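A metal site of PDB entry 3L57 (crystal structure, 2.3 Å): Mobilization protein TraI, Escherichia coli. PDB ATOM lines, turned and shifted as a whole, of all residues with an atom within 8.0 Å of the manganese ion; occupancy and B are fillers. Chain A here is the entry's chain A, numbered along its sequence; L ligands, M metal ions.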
ATOM      1  N   VAL A  16     -14.603  22.224  -4.344  1.00  0.00           N
ATOM      2  CA  VAL A  16     -15.620  22.945  -5.108  1.00  0.00           C
ATOM      3  C   VAL A  16     -16.391  23.896  -4.212  1.00  0.00           C
ATOM      4  O   VAL A  16     -16.770  23.527  -3.103  1.00  0.00           O
ATOM      5  CB  VAL A  16     -16.662  21.984  -5.727  1.00  0.00           C
ATOM      6  CG1 VAL A  16     -16.116  21.326  -6.973  1.00  0.00           C
ATOM      7  CG2 VAL A  16     -17.109  20.945  -4.696  1.00  0.00           C
ATOM      8  N   ASP A  84     -15.862  14.732  -1.273  1.00  0.00           N
ATOM      9  CA  ASP A  84     -16.390  15.072  -2.572  1.00  0.00           C
ATOM     10  C   ASP A  84     -16.656  13.794  -3.347  1.00  0.00           C
ATOM     11  O   ASP A  84     -15.733  13.107  -3.766  1.00  0.00           O
ATOM     12  CB  ASP A  84     -15.416  15.965  -3.344  1.00  0.00           C
ATOM     13  CG  ASP A  84     -15.910  16.311  -4.737  1.00  0.00           C
ATOM     14  OD1 ASP A  84     -16.881  15.676  -5.211  1.00  0.00           O
ATOM     15  OD2 ASP A  84     -15.347  17.223  -5.362  1.00  0.00           O
ATOM     16  N   THR A  86     -17.584  12.710  -6.665  1.00  0.00           N
ATOM     17  CA  THR A  86     -17.703  13.203  -8.037  1.00  0.00           C
ATOM     18  C   THR A  86     -18.235  12.104  -8.947  1.00  0.00           C
ATOM     19  O   THR A  86     -17.581  11.071  -9.146  1.00  0.00           O
ATOM     20  CB  THR A  86     -16.341  13.731  -8.536  1.00  0.00           C
ATOM     21  OG1 THR A  86     -15.848  14.713  -7.611  1.00  0.00           O
ATOM     22  CG2 THR A  86     -16.464  14.365  -9.922  1.00  0.00           C
ATOM     23  N   SER A  88     -19.274  11.037 -12.611  1.00  0.00           N
ATOM     24  CA  SER A  88     -18.996  11.393 -13.994  1.00  0.00           C
ATOM     25  C   SER A  88     -19.790  10.517 -14.955  1.00  0.00           C
ATOM     26  O   SER A  88     -19.848   9.305 -14.803  1.00  0.00           O
ATOM     27  CB  SER A  88     -17.497  11.256 -14.295  1.00  0.00           C
ATOM     28  OG  SER A  88     -16.737  12.109 -13.459  1.00  0.00           O
ATOM     29  N   PHE A 147     -22.607  20.437  -7.054  1.00  0.00           N
ATOM     30  CA  PHE A 147     -22.190  21.399  -8.062  1.00  0.00           C
ATOM     31  C   PHE A 147     -22.010  20.700  -9.393  1.00  0.00           C
ATOM     32  O   PHE A 147     -21.152  19.828  -9.528  1.00  0.00           O
ATOM     33  CB  PHE A 147     -20.852  22.040  -7.668  1.00  0.00           C
ATOM     34  CG  PHE A 147     -20.862  22.692  -6.321  1.00  0.00           C
ATOM     35  CD1 PHE A 147     -20.792  21.926  -5.166  1.00  0.00           C
ATOM     36  CD2 PHE A 147     -20.902  24.070  -6.212  1.00  0.00           C
ATOM     37  CE1 PHE A 147     -20.777  22.528  -3.925  1.00  0.00           C
ATOM     38  CE2 PHE A 147     -20.896  24.683  -4.967  1.00  0.00           C
ATOM     39  CZ  PHE A 147     -20.830  23.908  -3.821  1.00  0.00           C
ATOM     40  N   ARG A 148     -22.808  21.071 -10.383  1.00  0.00           N
ATOM     41  CA  ARG A 148     -22.695  20.430 -11.680  1.00  0.00           C
ATOM     42  C   ARG A 148     -21.708  21.169 -12.553  1.00  0.00           C
ATOM     43  O   ARG A 148     -21.770  22.393 -12.680  1.00  0.00           O
ATOM     44  CB  ARG A 148     -24.053  20.327 -12.385  1.00  0.00           C
ATOM     45  CG  ARG A 148     -23.955  19.623 -13.739  1.00  0.00           C
ATOM     46  CD  ARG A 148     -25.310  19.347 -14.348  1.00  0.00           C
ATOM     47  NE  ARG A 148     -25.943  20.558 -14.849  1.00  0.00           N
ATOM     48  CZ  ARG A 148     -27.032  21.099 -14.319  1.00  0.00           C
ATOM     49  NH1 ARG A 148     -27.553  22.207 -14.844  1.00  0.00           N
ATOM     50  NH2 ARG A 148     -27.613  20.532 -13.269  1.00  0.00           N
ATOM     51  N   HIS A 149     -20.789  20.420 -13.149  1.00  0.00           N
ATOM     52  CA  HIS A 149     -19.824  21.003 -14.066  1.00  0.00           C
ATOM     53  C   HIS A 149     -20.049  20.522 -15.489  1.00  0.00           C
ATOM     54  O   HIS A 149     -20.099  19.318 -15.766  1.00  0.00           O
ATOM     55  CB  HIS A 149     -18.401  20.711 -13.592  1.00  0.00           C
ATOM     56  CG  HIS A 149     -17.998  21.545 -12.407  1.00  0.00           C
ATOM     57  ND1 HIS A 149     -16.997  21.168 -11.545  1.00  0.00           N
ATOM     58  CD2 HIS A 149     -18.475  22.723 -11.944  1.00  0.00           C
ATOM     59  CE1 HIS A 149     -16.874  22.081 -10.592  1.00  0.00           C
ATOM     60  NE2 HIS A 149     -17.754  23.035 -10.825  1.00  0.00           N
ATOM     61  N   GLU A 150     -20.228  21.485 -16.389  1.00  0.00           N
ATOM     62  CA  GLU A 150     -20.464  21.189 -17.793  1.00  0.00           C
ATOM     63  C   GLU A 150     -19.267  21.639 -18.615  1.00  0.00           C
ATOM     64  O   GLU A 150     -19.259  22.735 -19.174  1.00  0.00           O
ATOM     65  CB  GLU A 150     -21.772  21.831 -18.264  1.00  0.00           C
ATOM     66  CG  GLU A 150     -22.984  21.335 -17.495  1.00  0.00           C
ATOM     67  CD  GLU A 150     -24.298  21.951 -17.958  1.00  0.00           C
ATOM     68  OE1 GLU A 150     -24.312  22.655 -18.991  1.00  0.00           O
ATOM     69  OE2 GLU A 150     -25.324  21.743 -17.275  1.00  0.00           O
ATOM     70  N   THR A 151     -18.250  20.786 -18.641  1.00  0.00           N
ATOM     71  CA  THR A 151     -17.003  21.049 -19.335  1.00  0.00           C
ATOM     72  C   THR A 151     -17.120  20.623 -20.794  1.00  0.00           C
ATOM     73  O   THR A 151     -16.955  19.447 -21.118  1.00  0.00           O
ATOM     74  CB  THR A 151     -15.844  20.252 -18.698  1.00  0.00           C
ATOM     75  OG1 THR A 151     -16.042  20.160 -17.277  1.00  0.00           O
ATOM     76  CG2 THR A 151     -14.507  20.916 -18.980  1.00  0.00           C
ATOM     77  N   ASP A 158     -17.025  16.417 -20.680  1.00  0.00           N
ATOM     78  CA  ASP A 158     -17.062  15.764 -19.380  1.00  0.00           C
ATOM     79  C   ASP A 158     -18.185  16.315 -18.493  1.00  0.00           C
ATOM     80  O   ASP A 158     -18.017  17.321 -17.814  1.00  0.00           O
ATOM     81  CB  ASP A 158     -15.712  15.911 -18.662  1.00  0.00           C
ATOM     82  CG  ASP A 158     -15.699  15.291 -17.282  1.00  0.00           C
ATOM     83  OD1 ASP A 158     -16.721  14.705 -16.867  1.00  0.00           O
ATOM     84  OD2 ASP A 158     -14.656  15.385 -16.603  1.00  0.00           O
ATOM     85  N   LEU A 159     -19.331  15.630 -18.504  1.00  0.00           N
ATOM     86  CA  LEU A 159     -20.426  15.990 -17.618  1.00  0.00           C
ATOM     87  C   LEU A 159     -20.253  15.270 -16.292  1.00  0.00           C
ATOM     88  O   LEU A 159     -20.249  14.041 -16.237  1.00  0.00           O
ATOM     89  CB  LEU A 159     -21.762  15.585 -18.234  1.00  0.00           C
ATOM     90  CG  LEU A 159     -23.004  15.723 -17.335  1.00  0.00           C
ATOM     91  CD1 LEU A 159     -23.321  17.192 -17.079  1.00  0.00           C
ATOM     92  CD2 LEU A 159     -24.188  15.025 -17.972  1.00  0.00           C
ATOM     93  N   HIS A 160     -20.107  16.031 -15.213  1.00  0.00           N
ATOM     94  CA  HIS A 160     -20.023  15.434 -13.899  1.00  0.00           C
ATOM     95  C   HIS A 160     -20.577  16.358 -12.834  1.00  0.00           C
ATOM     96  O   HIS A 160     -20.786  17.546 -13.070  1.00  0.00           O
ATOM     97  CB  HIS A 160     -18.575  15.057 -13.563  1.00  0.00           C
ATOM     98  CG  HIS A 160     -17.657  16.226 -13.453  1.00  0.00           C
ATOM     99  ND1 HIS A 160     -17.015  16.759 -14.538  1.00  0.00           N
ATOM    100  CD2 HIS A 160     -17.302  16.989 -12.389  1.00  0.00           C
ATOM    101  CE1 HIS A 160     -16.289  17.800 -14.152  1.00  0.00           C
ATOM    102  NE2 HIS A 160     -16.443  17.953 -12.855  1.00  0.00           N
ATOM    103  N   THR A 161     -20.818  15.799 -11.659  1.00  0.00           N
ATOM    104  CA  THR A 161     -21.334  16.569 -10.552  1.00  0.00           C
ATOM    105  C   THR A 161     -20.514  16.286  -9.299  1.00  0.00           C
ATOM    106  O   THR A 161     -20.212  15.140  -8.995  1.00  0.00           O
ATOM    107  CB  THR A 161     -22.835  16.267 -10.303  1.00  0.00           C
ATOM    108  OG1 THR A 161     -23.619  16.891 -11.327  1.00  0.00           O
ATOM    109  CG2 THR A 161     -23.266  16.784  -8.951  1.00  0.00           C
ATOM    110  N   HIS A 162     -20.124  17.343  -8.596  1.00  0.00           N
ATOM    111  CA  HIS A 162     -19.503  17.197  -7.293  1.00  0.00           C
ATOM    112  C   HIS A 162     -20.594  17.178  -6.224  1.00  0.00           C
ATOM    113  O   HIS A 162     -21.239  18.197  -5.972  1.00  0.00           O
ATOM    114  CB  HIS A 162     -18.538  18.350  -7.004  1.00  0.00           C
ATOM    115  CG  HIS A 162     -17.422  18.455  -7.989  1.00  0.00           C
ATOM    116  ND1 HIS A 162     -16.148  17.978  -7.721  1.00  0.00           N
ATOM    117  CD2 HIS A 162     -17.366  18.996  -9.224  1.00  0.00           C
ATOM    118  CE1 HIS A 162     -15.370  18.224  -8.756  1.00  0.00           C
ATOM    119  NE2 HIS A 162     -16.084  18.835  -9.685  1.00  0.00           N
HETATM  120  C1  LIG L   1     -12.342  16.227 -12.540  1.00  0.00           C
HETATM  121  O1  LIG L   1     -13.445  15.821 -12.339  1.00  0.00           O
HETATM  122  O2  LIG L   1     -11.291  15.313 -12.699  1.00  0.00           O
HETATM  123  C2  LIG L   1     -12.159  17.644 -13.078  1.00  0.00           C
HETATM  124  C3  LIG L   1     -12.649  18.821 -12.235  1.00  0.00           C
HETATM  125  O3  LIG L   1     -13.685  18.388 -11.416  1.00  0.00           O
HETATM  126  C4  LIG L   1     -11.548  19.360 -11.320  1.00  0.00           C
HETATM  127  C5  LIG L   1     -11.999  20.517 -10.445  1.00  0.00           C
HETATM  128  O4  LIG L   1     -13.293  21.037 -10.602  1.00  0.00           O
HETATM  129  O5  LIG L   1     -11.353  20.831  -9.497  1.00  0.00           O
HETATM  130  C6  LIG L   1     -13.111  19.953 -13.158  1.00  0.00           C
HETATM  131  O6  LIG L   1     -14.462  20.279 -13.273  1.00  0.00           O
HETATM  132  O7  LIG L   1     -12.327  20.477 -13.879  1.00  0.00           O
HETATM  133 MN    MN M   1     -15.609  19.500 -11.610  1.00  0.00          MN
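The backbone carbonyl oxygen (O) of His 162 sits at hydrogen-bond distance from the backbone NH (N) of Phe 147, at 2.8 Å.
OD2 of Asp 84 is in hydrogen-bond range of ND1 of His 162 (2.6 Å).
A ring nitrogen (ND1) of His 162 is in hydrogen-bond range of the side-chain hydroxyl of Thr 86.
The side-chain carboxylate of Asp 158 lies within hydrogen-bond range of a ring nitrogen (ND1) of His 160 (3.1 Å).
Within 4 Å of the manganese ion: His 149, His 160 and His 162.
The nearest printed residue that does not touch the manganese ion is Val 16 (5.0 Å).
The manganese ion is bound by a ring nitrogen (NE2) of His 162 (2.1 Å), a ring nitrogen (NE2) of His 160 (2.2 Å), an oxygen (O6) of the ligand (2.2 Å), a ring nitrogen (ND1) of His 149 (2.2 Å) and an oxygen (O3) of the ligand (2.2 Å).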
